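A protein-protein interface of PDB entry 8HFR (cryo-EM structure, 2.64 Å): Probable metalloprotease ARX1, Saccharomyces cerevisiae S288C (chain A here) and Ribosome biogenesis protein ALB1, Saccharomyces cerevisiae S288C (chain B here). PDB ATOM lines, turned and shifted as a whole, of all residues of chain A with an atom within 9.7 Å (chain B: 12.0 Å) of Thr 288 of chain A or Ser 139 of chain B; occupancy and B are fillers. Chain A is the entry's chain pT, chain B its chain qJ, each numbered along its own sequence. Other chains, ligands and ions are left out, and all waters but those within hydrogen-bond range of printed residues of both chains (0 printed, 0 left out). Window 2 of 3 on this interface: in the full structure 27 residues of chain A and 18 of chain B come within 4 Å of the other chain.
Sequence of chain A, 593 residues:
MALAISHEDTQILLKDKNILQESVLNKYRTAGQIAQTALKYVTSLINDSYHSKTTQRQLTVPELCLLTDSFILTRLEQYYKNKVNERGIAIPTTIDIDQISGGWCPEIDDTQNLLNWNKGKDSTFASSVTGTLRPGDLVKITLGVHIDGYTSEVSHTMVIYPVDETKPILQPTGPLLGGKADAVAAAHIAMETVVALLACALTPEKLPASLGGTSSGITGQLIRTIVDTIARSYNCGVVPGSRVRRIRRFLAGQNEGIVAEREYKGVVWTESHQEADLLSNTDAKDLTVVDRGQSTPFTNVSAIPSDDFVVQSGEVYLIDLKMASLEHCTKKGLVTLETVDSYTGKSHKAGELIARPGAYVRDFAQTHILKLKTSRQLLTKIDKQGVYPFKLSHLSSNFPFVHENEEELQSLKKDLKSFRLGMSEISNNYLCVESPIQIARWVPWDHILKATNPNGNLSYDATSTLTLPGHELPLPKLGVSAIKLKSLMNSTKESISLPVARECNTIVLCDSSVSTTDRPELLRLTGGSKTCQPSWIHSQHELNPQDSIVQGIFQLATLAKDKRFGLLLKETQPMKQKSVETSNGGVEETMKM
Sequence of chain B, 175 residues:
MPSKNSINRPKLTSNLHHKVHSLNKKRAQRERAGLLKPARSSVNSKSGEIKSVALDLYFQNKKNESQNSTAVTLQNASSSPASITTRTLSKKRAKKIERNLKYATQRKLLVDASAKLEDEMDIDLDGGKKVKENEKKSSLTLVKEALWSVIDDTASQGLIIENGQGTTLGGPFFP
N of Leu 478 of chain A sits at hydrogen-bond distance from OE2 of Glu 275 of chain A, at 3.2 Å.
Val 143 of chain B touches Leu 279 of chain A.
Leu 147 of chain B touches Leu 279 of chain A.
CG2 of Thr 288 of chain A touches OG of Ser 139 of chain B, 3.6 Å away.
Lys 477 of chain A touches Val 143 of chain B (O to CG1, 3.9 Å).
Leu 478 of chain A touches Leu 140 of chain B.
CG1 of Val 143 of chain B touches CD1 of Leu 478 of chain A, at 3.8 Å.
Lys 144 of chain B touches Leu 478 of chain A.
Thr 288 of chain A touches just one residue of chain B: Ser 139 (3.6 Å).
Ser 139 of chain B touches just one residue of chain A: Thr 288.
No residue of chain B comes within 4 Å of Asp 286 of chain A.
No residue of chain B comes within 4 Å of Leu 287 of chain A.
No residue of chain B comes within 4 Å of Val 289 of chain A.
Of chain B, only Val 143 (3.9 Å) comes within 4 Å of Lys 477 of chain A.
No residue of chain A comes within 4 Å of Ser 138 of chain B.
No residue of chain A comes within 4 Å of Thr 141 of chain B.
No residue of chain A comes within 4 Å of Leu 142 of chain B.
Of the printed residues of chain B, Leu 478 of chain A touches Leu 140, Val 143 and Lys 144.
Printed residues of chain A within 4 Å of Leu 140 of chain B: Leu 478.
Glu 145 of chain B touches none of the printed residues of chain A.
The nearest residue of chain B that does not touch Thr 288 of chain A is Val 143 of chain B (4.4 Å).
The nearest residue of chain A that does not touch Ser 139 of chain B is Val 289 of chain A (5.5 Å).
The nearest printed residue of chain A that does not touch Leu 147 of chain B is Glu 275 of chain A (5.3 Å).
Hydrophobic or aromatic side chains of chain A that line the printed part of chain B: Leu 279 and Leu 478.
Along chain A the printed residues that touch a printed residue of chain B span positions 279 to 478.
Of the 14 printed residues of chain B, 5 touch a printed residue of chain A.
Among the printed residues, 7 pairs touch across the chains.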
ATOM      1  N   GLU A 275      -8.998   2.758  -8.685  1.00  0.00           N
ATOM      2  CA  GLU A 275      -9.765   3.771  -7.968  1.00  0.00           C
ATOM      3  C   GLU A 275      -9.016   5.096  -7.907  1.00  0.00           C
ATOM      4  O   GLU A 275      -9.612   6.164  -8.092  1.00  0.00           O
ATOM      5  CB  GLU A 275     -10.082   3.275  -6.561  1.00  0.00           C
ATOM      6  CG  GLU A 275     -10.890   4.237  -5.718  1.00  0.00           C
ATOM      7  CD  GLU A 275     -10.598   4.092  -4.234  1.00  0.00           C
ATOM      8  OE1 GLU A 275      -9.468   3.708  -3.873  1.00  0.00           O
ATOM      9  OE2 GLU A 275     -11.505   4.358  -3.425  1.00  0.00           O
ATOM     10  N   LEU A 279     -10.114   8.587  -9.642  1.00  0.00           N
ATOM     11  CA  LEU A 279     -10.423   9.716  -8.772  1.00  0.00           C
ATOM     12  C   LEU A 279      -9.554  10.924  -9.092  1.00  0.00           C
ATOM     13  O   LEU A 279     -10.031  12.063  -9.056  1.00  0.00           O
ATOM     14  CB  LEU A 279     -10.234   9.286  -7.320  1.00  0.00           C
ATOM     15  CG  LEU A 279     -10.916  10.005  -6.162  1.00  0.00           C
ATOM     16  CD1 LEU A 279     -11.113   9.008  -5.043  1.00  0.00           C
ATOM     17  CD2 LEU A 279     -10.101  11.173  -5.673  1.00  0.00           C
ATOM     18  N   ALA A 284      -8.776  16.041  -5.805  1.00  0.00           N
ATOM     19  CA  ALA A 284      -9.360  15.315  -4.676  1.00  0.00           C
ATOM     20  C   ALA A 284      -8.494  14.166  -4.185  1.00  0.00           C
ATOM     21  O   ALA A 284      -8.982  13.309  -3.444  1.00  0.00           O
ATOM     22  CB  ALA A 284     -10.775  14.800  -4.981  1.00  0.00           C
ATOM     23  N   LYS A 285      -7.217  14.138  -4.546  1.00  0.00           N
ATOM     24  CA  LYS A 285      -6.287  13.122  -4.057  1.00  0.00           C
ATOM     25  C   LYS A 285      -5.676  13.533  -2.718  1.00  0.00           C
ATOM     26  O   LYS A 285      -4.462  13.694  -2.591  1.00  0.00           O
ATOM     27  CB  LYS A 285      -5.208  12.870  -5.102  1.00  0.00           C
ATOM     28  N   ASP A 286      -6.516  13.709  -1.701  1.00  0.00           N
ATOM     29  CA  ASP A 286      -6.067  14.290  -0.443  1.00  0.00           C
ATOM     30  C   ASP A 286      -5.987  13.290   0.704  1.00  0.00           C
ATOM     31  O   ASP A 286      -5.510  13.666   1.779  1.00  0.00           O
ATOM     32  CB  ASP A 286      -6.976  15.457  -0.053  1.00  0.00           C
ATOM     33  CG  ASP A 286      -8.441  15.083  -0.056  1.00  0.00           C
ATOM     34  OD1 ASP A 286      -8.786  14.025  -0.620  1.00  0.00           O
ATOM     35  OD2 ASP A 286      -9.252  15.853   0.502  1.00  0.00           O
ATOM     36  N   LEU A 287      -6.427  12.043   0.489  1.00  0.00           N
ATOM     37  CA  LEU A 287      -6.313  10.919   1.431  1.00  0.00           C
ATOM     38  C   LEU A 287      -7.036  11.217   2.750  1.00  0.00           C
ATOM     39  O   LEU A 287      -6.437  11.414   3.808  1.00  0.00           O
ATOM     40  CB  LEU A 287      -4.843  10.537   1.658  1.00  0.00           C
ATOM     41  CG  LEU A 287      -4.068  10.160   0.390  1.00  0.00           C
ATOM     42  CD1 LEU A 287      -2.604   9.869   0.690  1.00  0.00           C
ATOM     43  CD2 LEU A 287      -4.719   8.978  -0.305  1.00  0.00           C
ATOM     44  N   THR A 288      -8.362  11.258   2.637  1.00  0.00           N
ATOM     45  CA  THR A 288      -9.257  11.671   3.710  1.00  0.00           C
ATOM     46  C   THR A 288      -9.510  10.546   4.714  1.00  0.00           C
ATOM     47  O   THR A 288      -9.301  10.712   5.920  1.00  0.00           O
ATOM     48  CB  THR A 288     -10.586  12.140   3.132  1.00  0.00           C
ATOM     49  OG1 THR A 288     -11.133  11.111   2.300  1.00  0.00           O
ATOM     50  CG2 THR A 288     -10.403  13.380   2.316  1.00  0.00           C
ATOM     51  N   VAL A 289     -10.003   9.404   4.219  1.00  0.00           N
ATOM     52  CA  VAL A 289     -10.664   8.360   5.009  1.00  0.00           C
ATOM     53  C   VAL A 289      -9.712   7.734   6.023  1.00  0.00           C
ATOM     54  O   VAL A 289      -8.540   7.486   5.721  1.00  0.00           O
ATOM     55  CB  VAL A 289     -11.265   7.292   4.071  1.00  0.00           C
ATOM     56  CG1 VAL A 289     -12.182   6.334   4.821  1.00  0.00           C
ATOM     57  CG2 VAL A 289     -12.033   7.956   2.959  1.00  0.00           C
ATOM     58  N   VAL A 290     -10.200   7.506   7.244  1.00  0.00           N
ATOM     59  CA  VAL A 290      -9.378   6.997   8.338  1.00  0.00           C
ATOM     60  C   VAL A 290      -9.025   5.533   8.111  1.00  0.00           C
ATOM     61  O   VAL A 290      -9.585   4.874   7.230  1.00  0.00           O
ATOM     62  CB  VAL A 290     -10.074   7.181   9.695  1.00  0.00           C
ATOM     63  CG1 VAL A 290     -10.150   8.650  10.043  1.00  0.00           C
ATOM     64  CG2 VAL A 290     -11.457   6.550   9.672  1.00  0.00           C
ATOM     65  N   ASP A 291      -8.091   5.023   8.908  1.00  0.00           N
ATOM     66  CA  ASP A 291      -7.529   3.700   8.700  1.00  0.00           C
ATOM     67  C   ASP A 291      -8.328   2.660   9.477  1.00  0.00           C
ATOM     68  O   ASP A 291      -9.364   2.958  10.072  1.00  0.00           O
ATOM     69  CB  ASP A 291      -6.065   3.688   9.114  1.00  0.00           C
ATOM     70  CG  ASP A 291      -5.323   4.892   8.609  1.00  0.00           C
ATOM     71  OD1 ASP A 291      -5.758   5.460   7.588  1.00  0.00           O
ATOM     72  OD2 ASP A 291      -4.318   5.281   9.237  1.00  0.00           O
ATOM     73  N   ASN A 457     -15.451  -0.059   6.828  1.00  0.00           N
ATOM     74  CA  ASN A 457     -14.023  -0.292   6.954  1.00  0.00           C
ATOM     75  C   ASN A 457     -13.694  -1.534   7.766  1.00  0.00           C
ATOM     76  O   ASN A 457     -12.586  -2.057   7.642  1.00  0.00           O
ATOM     77  CB  ASN A 457     -13.384   0.928   7.621  1.00  0.00           C
ATOM     78  CG  ASN A 457     -11.979   1.125   7.216  1.00  0.00           C
ATOM     79  OD1 ASN A 457     -11.448   0.367   6.422  1.00  0.00           O
ATOM     80  ND2 ASN A 457     -11.359   2.177   7.728  1.00  0.00           N
ATOM     81  N   PRO A 476      -9.616   1.353  -0.725  1.00  0.00           N
ATOM     82  CA  PRO A 476      -9.426   1.826   0.654  1.00  0.00           C
ATOM     83  C   PRO A 476     -10.118   3.141   0.962  1.00  0.00           C
ATOM     84  O   PRO A 476     -10.730   3.266   2.028  1.00  0.00           O
ATOM     85  CB  PRO A 476      -7.901   1.945   0.765  1.00  0.00           C
ATOM     86  CG  PRO A 476      -7.428   2.163  -0.620  1.00  0.00           C
ATOM     87  CD  PRO A 476      -8.405   1.515  -1.547  1.00  0.00           C
ATOM     88  N   LYS A 477     -10.041   4.130   0.073  1.00  0.00           N
ATOM     89  CA  LYS A 477     -10.621   5.440   0.324  1.00  0.00           C
ATOM     90  C   LYS A 477     -12.052   5.545  -0.173  1.00  0.00           C
ATOM     91  O   LYS A 477     -12.566   6.653  -0.347  1.00  0.00           O
ATOM     92  CB  LYS A 477      -9.751   6.537  -0.293  1.00  0.00           C
ATOM     93  CG  LYS A 477      -9.603   6.471  -1.791  1.00  0.00           C
ATOM     94  CD  LYS A 477      -8.972   7.731  -2.323  1.00  0.00           C
ATOM     95  CE  LYS A 477      -7.473   7.585  -2.477  1.00  0.00           C
ATOM     96  NZ  LYS A 477      -6.953   8.486  -3.545  1.00  0.00           N
ATOM     97  N   LEU A 478     -12.698   4.412  -0.410  1.00  0.00           N
ATOM     98  CA  LEU A 478     -14.133   4.341  -0.606  1.00  0.00           C
ATOM     99  C   LEU A 478     -14.819   3.484   0.444  1.00  0.00           C
ATOM    100  O   LEU A 478     -16.026   3.635   0.646  1.00  0.00           O
ATOM    101  CB  LEU A 478     -14.447   3.794  -2.006  1.00  0.00           C
ATOM    102  CG  LEU A 478     -15.785   4.106  -2.659  1.00  0.00           C
ATOM    103  CD1 LEU A 478     -16.029   5.596  -2.675  1.00  0.00           C
ATOM    104  CD2 LEU A 478     -15.761   3.567  -4.070  1.00  0.00           C
ATOM    105  N   GLY A 479     -14.083   2.608   1.123  1.00  0.00           N
ATOM    106  CA  GLY A 479     -14.605   1.859   2.245  1.00  0.00           C
ATOM    107  C   GLY A 479     -15.224   0.535   1.860  1.00  0.00           C
ATOM    108  O   GLY A 479     -16.224   0.119   2.449  1.00  0.00           O
ATOM    109  N   GLU B 135     -23.972  23.255   5.805  1.00  0.00           N
ATOM    110  CA  GLU B 135     -23.790  21.867   6.216  1.00  0.00           C
ATOM    111  C   GLU B 135     -22.306  21.548   6.127  1.00  0.00           C
ATOM    112  O   GLU B 135     -21.523  22.307   5.549  1.00  0.00           O
ATOM    113  CB  GLU B 135     -24.580  20.879   5.341  1.00  0.00           C
ATOM    114  N   LYS B 136     -21.932  20.413   6.710  1.00  0.00           N
ATOM    115  CA  LYS B 136     -20.590  19.859   6.558  1.00  0.00           C
ATOM    116  C   LYS B 136     -20.740  18.440   6.020  1.00  0.00           C
ATOM    117  O   LYS B 136     -20.942  17.478   6.760  1.00  0.00           O
ATOM    118  CB  LYS B 136     -19.833  19.896   7.881  1.00  0.00           C
ATOM    119  N   LYS B 137     -20.661  18.323   4.695  1.00  0.00           N
ATOM    120  CA  LYS B 137     -20.767  17.018   4.060  1.00  0.00           C
ATOM    121  C   LYS B 137     -19.511  16.200   4.324  1.00  0.00           C
ATOM    122  O   LYS B 137     -18.392  16.722   4.296  1.00  0.00           O
ATOM    123  CB  LYS B 137     -20.992  17.175   2.558  1.00  0.00           C
ATOM    124  N   SER B 138     -19.705  14.911   4.590  1.00  0.00           N
ATOM    125  CA  SER B 138     -18.605  14.035   4.953  1.00  0.00           C
ATOM    126  C   SER B 138     -17.707  13.760   3.750  1.00  0.00           C
ATOM    127  O   SER B 138     -18.087  13.953   2.590  1.00  0.00           O
ATOM    128  CB  SER B 138     -19.134  12.720   5.530  1.00  0.00           C
ATOM    129  OG  SER B 138     -18.094  11.956   6.115  1.00  0.00           O
ATOM    130  N   SER B 139     -16.488  13.309   4.051  1.00  0.00           N
ATOM    131  CA  SER B 139     -15.500  13.095   3.004  1.00  0.00           C
ATOM    132  C   SER B 139     -15.832  11.881   2.153  1.00  0.00           C
ATOM    133  O   SER B 139     -15.446  11.831   0.979  1.00  0.00           O
ATOM    134  CB  SER B 139     -14.117  12.950   3.616  1.00  0.00           C
ATOM    135  OG  SER B 139     -13.537  14.217   3.860  1.00  0.00           O
ATOM    136  N   LEU B 140     -16.551  10.908   2.723  1.00  0.00           N
ATOM    137  CA  LEU B 140     -17.122   9.830   1.923  1.00  0.00           C
ATOM    138  C   LEU B 140     -18.067  10.382   0.870  1.00  0.00           C
ATOM    139  O   LEU B 140     -17.976  10.009  -0.300  1.00  0.00           O
ATOM    140  CB  LEU B 140     -17.849   8.829   2.820  1.00  0.00           C
ATOM    141  CG  LEU B 140     -18.261   7.500   2.171  1.00  0.00           C
ATOM    142  CD1 LEU B 140     -17.048   6.632   1.901  1.00  0.00           C
ATOM    143  CD2 LEU B 140     -19.265   6.754   3.027  1.00  0.00           C
ATOM    144  N   THR B 141     -18.933  11.326   1.254  1.00  0.00           N
ATOM    145  CA  THR B 141     -19.861  11.942   0.308  1.00  0.00           C
ATOM    146  C   THR B 141     -19.131  12.783  -0.729  1.00  0.00           C
ATOM    147  O   THR B 141     -19.547  12.832  -1.893  1.00  0.00           O
ATOM    148  CB  THR B 141     -20.868  12.808   1.051  1.00  0.00           C
ATOM    149  OG1 THR B 141     -20.244  14.051   1.395  1.00  0.00           O
ATOM    150  CG2 THR B 141     -21.324  12.120   2.315  1.00  0.00           C
ATOM    151  N   LEU B 142     -18.046  13.450  -0.321  1.00  0.00           N
ATOM    152  CA  LEU B 142     -17.234  14.217  -1.266  1.00  0.00           C
ATOM    153  C   LEU B 142     -16.595  13.311  -2.314  1.00  0.00           C
ATOM    154  O   LEU B 142     -16.598  13.633  -3.509  1.00  0.00           O
ATOM    155  CB  LEU B 142     -16.158  15.002  -0.517  1.00  0.00           C
ATOM    156  CG  LEU B 142     -16.568  16.154   0.406  1.00  0.00           C
ATOM    157  CD1 LEU B 142     -15.379  17.066   0.638  1.00  0.00           C
ATOM    158  CD2 LEU B 142     -17.747  16.945  -0.138  1.00  0.00           C
ATOM    159  N   VAL B 143     -16.074  12.160  -1.882  1.00  0.00           N
ATOM    160  CA  VAL B 143     -15.491  11.200  -2.817  1.00  0.00           C
ATOM    161  C   VAL B 143     -16.571  10.594  -3.713  1.00  0.00           C
ATOM    162  O   VAL B 143     -16.355  10.405  -4.917  1.00  0.00           O
ATOM    163  CB  VAL B 143     -14.699  10.133  -2.039  1.00  0.00           C
ATOM    164  CG1 VAL B 143     -14.265   8.983  -2.930  1.00  0.00           C
ATOM    165  CG2 VAL B 143     -13.477  10.755  -1.417  1.00  0.00           C
ATOM    166  N   LYS B 144     -17.765  10.344  -3.160  1.00  0.00           N
ATOM    167  CA  LYS B 144     -18.851   9.762  -3.952  1.00  0.00           C
ATOM    168  C   LYS B 144     -19.322  10.717  -5.040  1.00  0.00           C
ATOM    169  O   LYS B 144     -19.516  10.309  -6.189  1.00  0.00           O
ATOM    170  CB  LYS B 144     -20.025   9.354  -3.056  1.00  0.00           C
ATOM    171  CG  LYS B 144     -19.762   8.161  -2.143  1.00  0.00           C
ATOM    172  CD  LYS B 144     -19.704   6.842  -2.861  1.00  0.00           C
ATOM    173  CE  LYS B 144     -21.074   6.216  -2.959  1.00  0.00           C
ATOM    174  NZ  LYS B 144     -21.568   5.781  -1.620  1.00  0.00           N
ATOM    175  N   GLU B 145     -19.464  12.008  -4.718  1.00  0.00           N
ATOM    176  CA  GLU B 145     -19.895  12.955  -5.746  1.00  0.00           C
ATOM    177  C   GLU B 145     -18.783  13.237  -6.751  1.00  0.00           C
ATOM    178  O   GLU B 145     -19.056  13.437  -7.945  1.00  0.00           O
ATOM    179  CB  GLU B 145     -20.415  14.250  -5.114  1.00  0.00           C
ATOM    180  CG  GLU B 145     -19.431  15.057  -4.270  1.00  0.00           C
ATOM    181  CD  GLU B 145     -18.667  16.105  -5.068  1.00  0.00           C
ATOM    182  OE1 GLU B 145     -19.049  16.377  -6.223  1.00  0.00           O
ATOM    183  OE2 GLU B 145     -17.682  16.657  -4.539  1.00  0.00           O
ATOM    184  N   ALA B 146     -17.519  13.221  -6.306  1.00  0.00           N
ATOM    185  CA  ALA B 146     -16.415  13.450  -7.233  1.00  0.00           C
ATOM    186  C   ALA B 146     -16.241  12.276  -8.192  1.00  0.00           C
ATOM    187  O   ALA B 146     -15.795  12.458  -9.330  1.00  0.00           O
ATOM    188  CB  ALA B 146     -15.126  13.714  -6.457  1.00  0.00           C
ATOM    189  N   LEU B 147     -16.585  11.063  -7.750  1.00  0.00           N
ATOM    190  CA  LEU B 147     -16.638   9.930  -8.667  1.00  0.00           C
ATOM    191  C   LEU B 147     -17.872   9.978  -9.554  1.00  0.00           C
ATOM    192  O   LEU B 147     -17.820   9.527 -10.706  1.00  0.00           O
ATOM    193  CB  LEU B 147     -16.621   8.612  -7.895  1.00  0.00           C
ATOM    194  CG  LEU B 147     -15.312   7.872  -7.628  1.00  0.00           C
ATOM    195  CD1 LEU B 147     -14.705   7.453  -8.940  1.00  0.00           C
ATOM    196  CD2 LEU B 147     -14.332   8.683  -6.836  1.00  0.00           C
ATOM    197  N   TRP B 148     -18.990  10.485  -9.020  1.00  0.00           N
ATOM    198  CA  TRP B 148     -20.239  10.513  -9.769  1.00  0.00           C
ATOM    199  C   TRP B 148     -20.146  11.455 -10.952  1.00  0.00           C
ATOM    200  O   TRP B 148     -20.709  11.172 -12.014  1.00  0.00           O
ATOM    201  CB  TRP B 148     -21.397  10.926  -8.862  1.00  0.00           C
ATOM    202  CG  TRP B 148     -22.201   9.789  -8.325  1.00  0.00           C
ATOM    203  CD1 TRP B 148     -22.373   9.459  -7.016  1.00  0.00           C
ATOM    204  CD2 TRP B 148     -22.955   8.831  -9.081  1.00  0.00           C
ATOM    205  NE1 TRP B 148     -23.175   8.352  -6.906  1.00  0.00           N
ATOM    206  CE2 TRP B 148     -23.547   7.947  -8.159  1.00  0.00           C
ATOM    207  CE3 TRP B 148     -23.184   8.632 -10.446  1.00  0.00           C
ATOM    208  CZ2 TRP B 148     -24.349   6.886  -8.555  1.00  0.00           C
ATOM    209  CZ3 TRP B 148     -23.979   7.575 -10.836  1.00  0.00           C
ATOM    210  CH2 TRP B 148     -24.553   6.716  -9.895  1.00  0.00           C
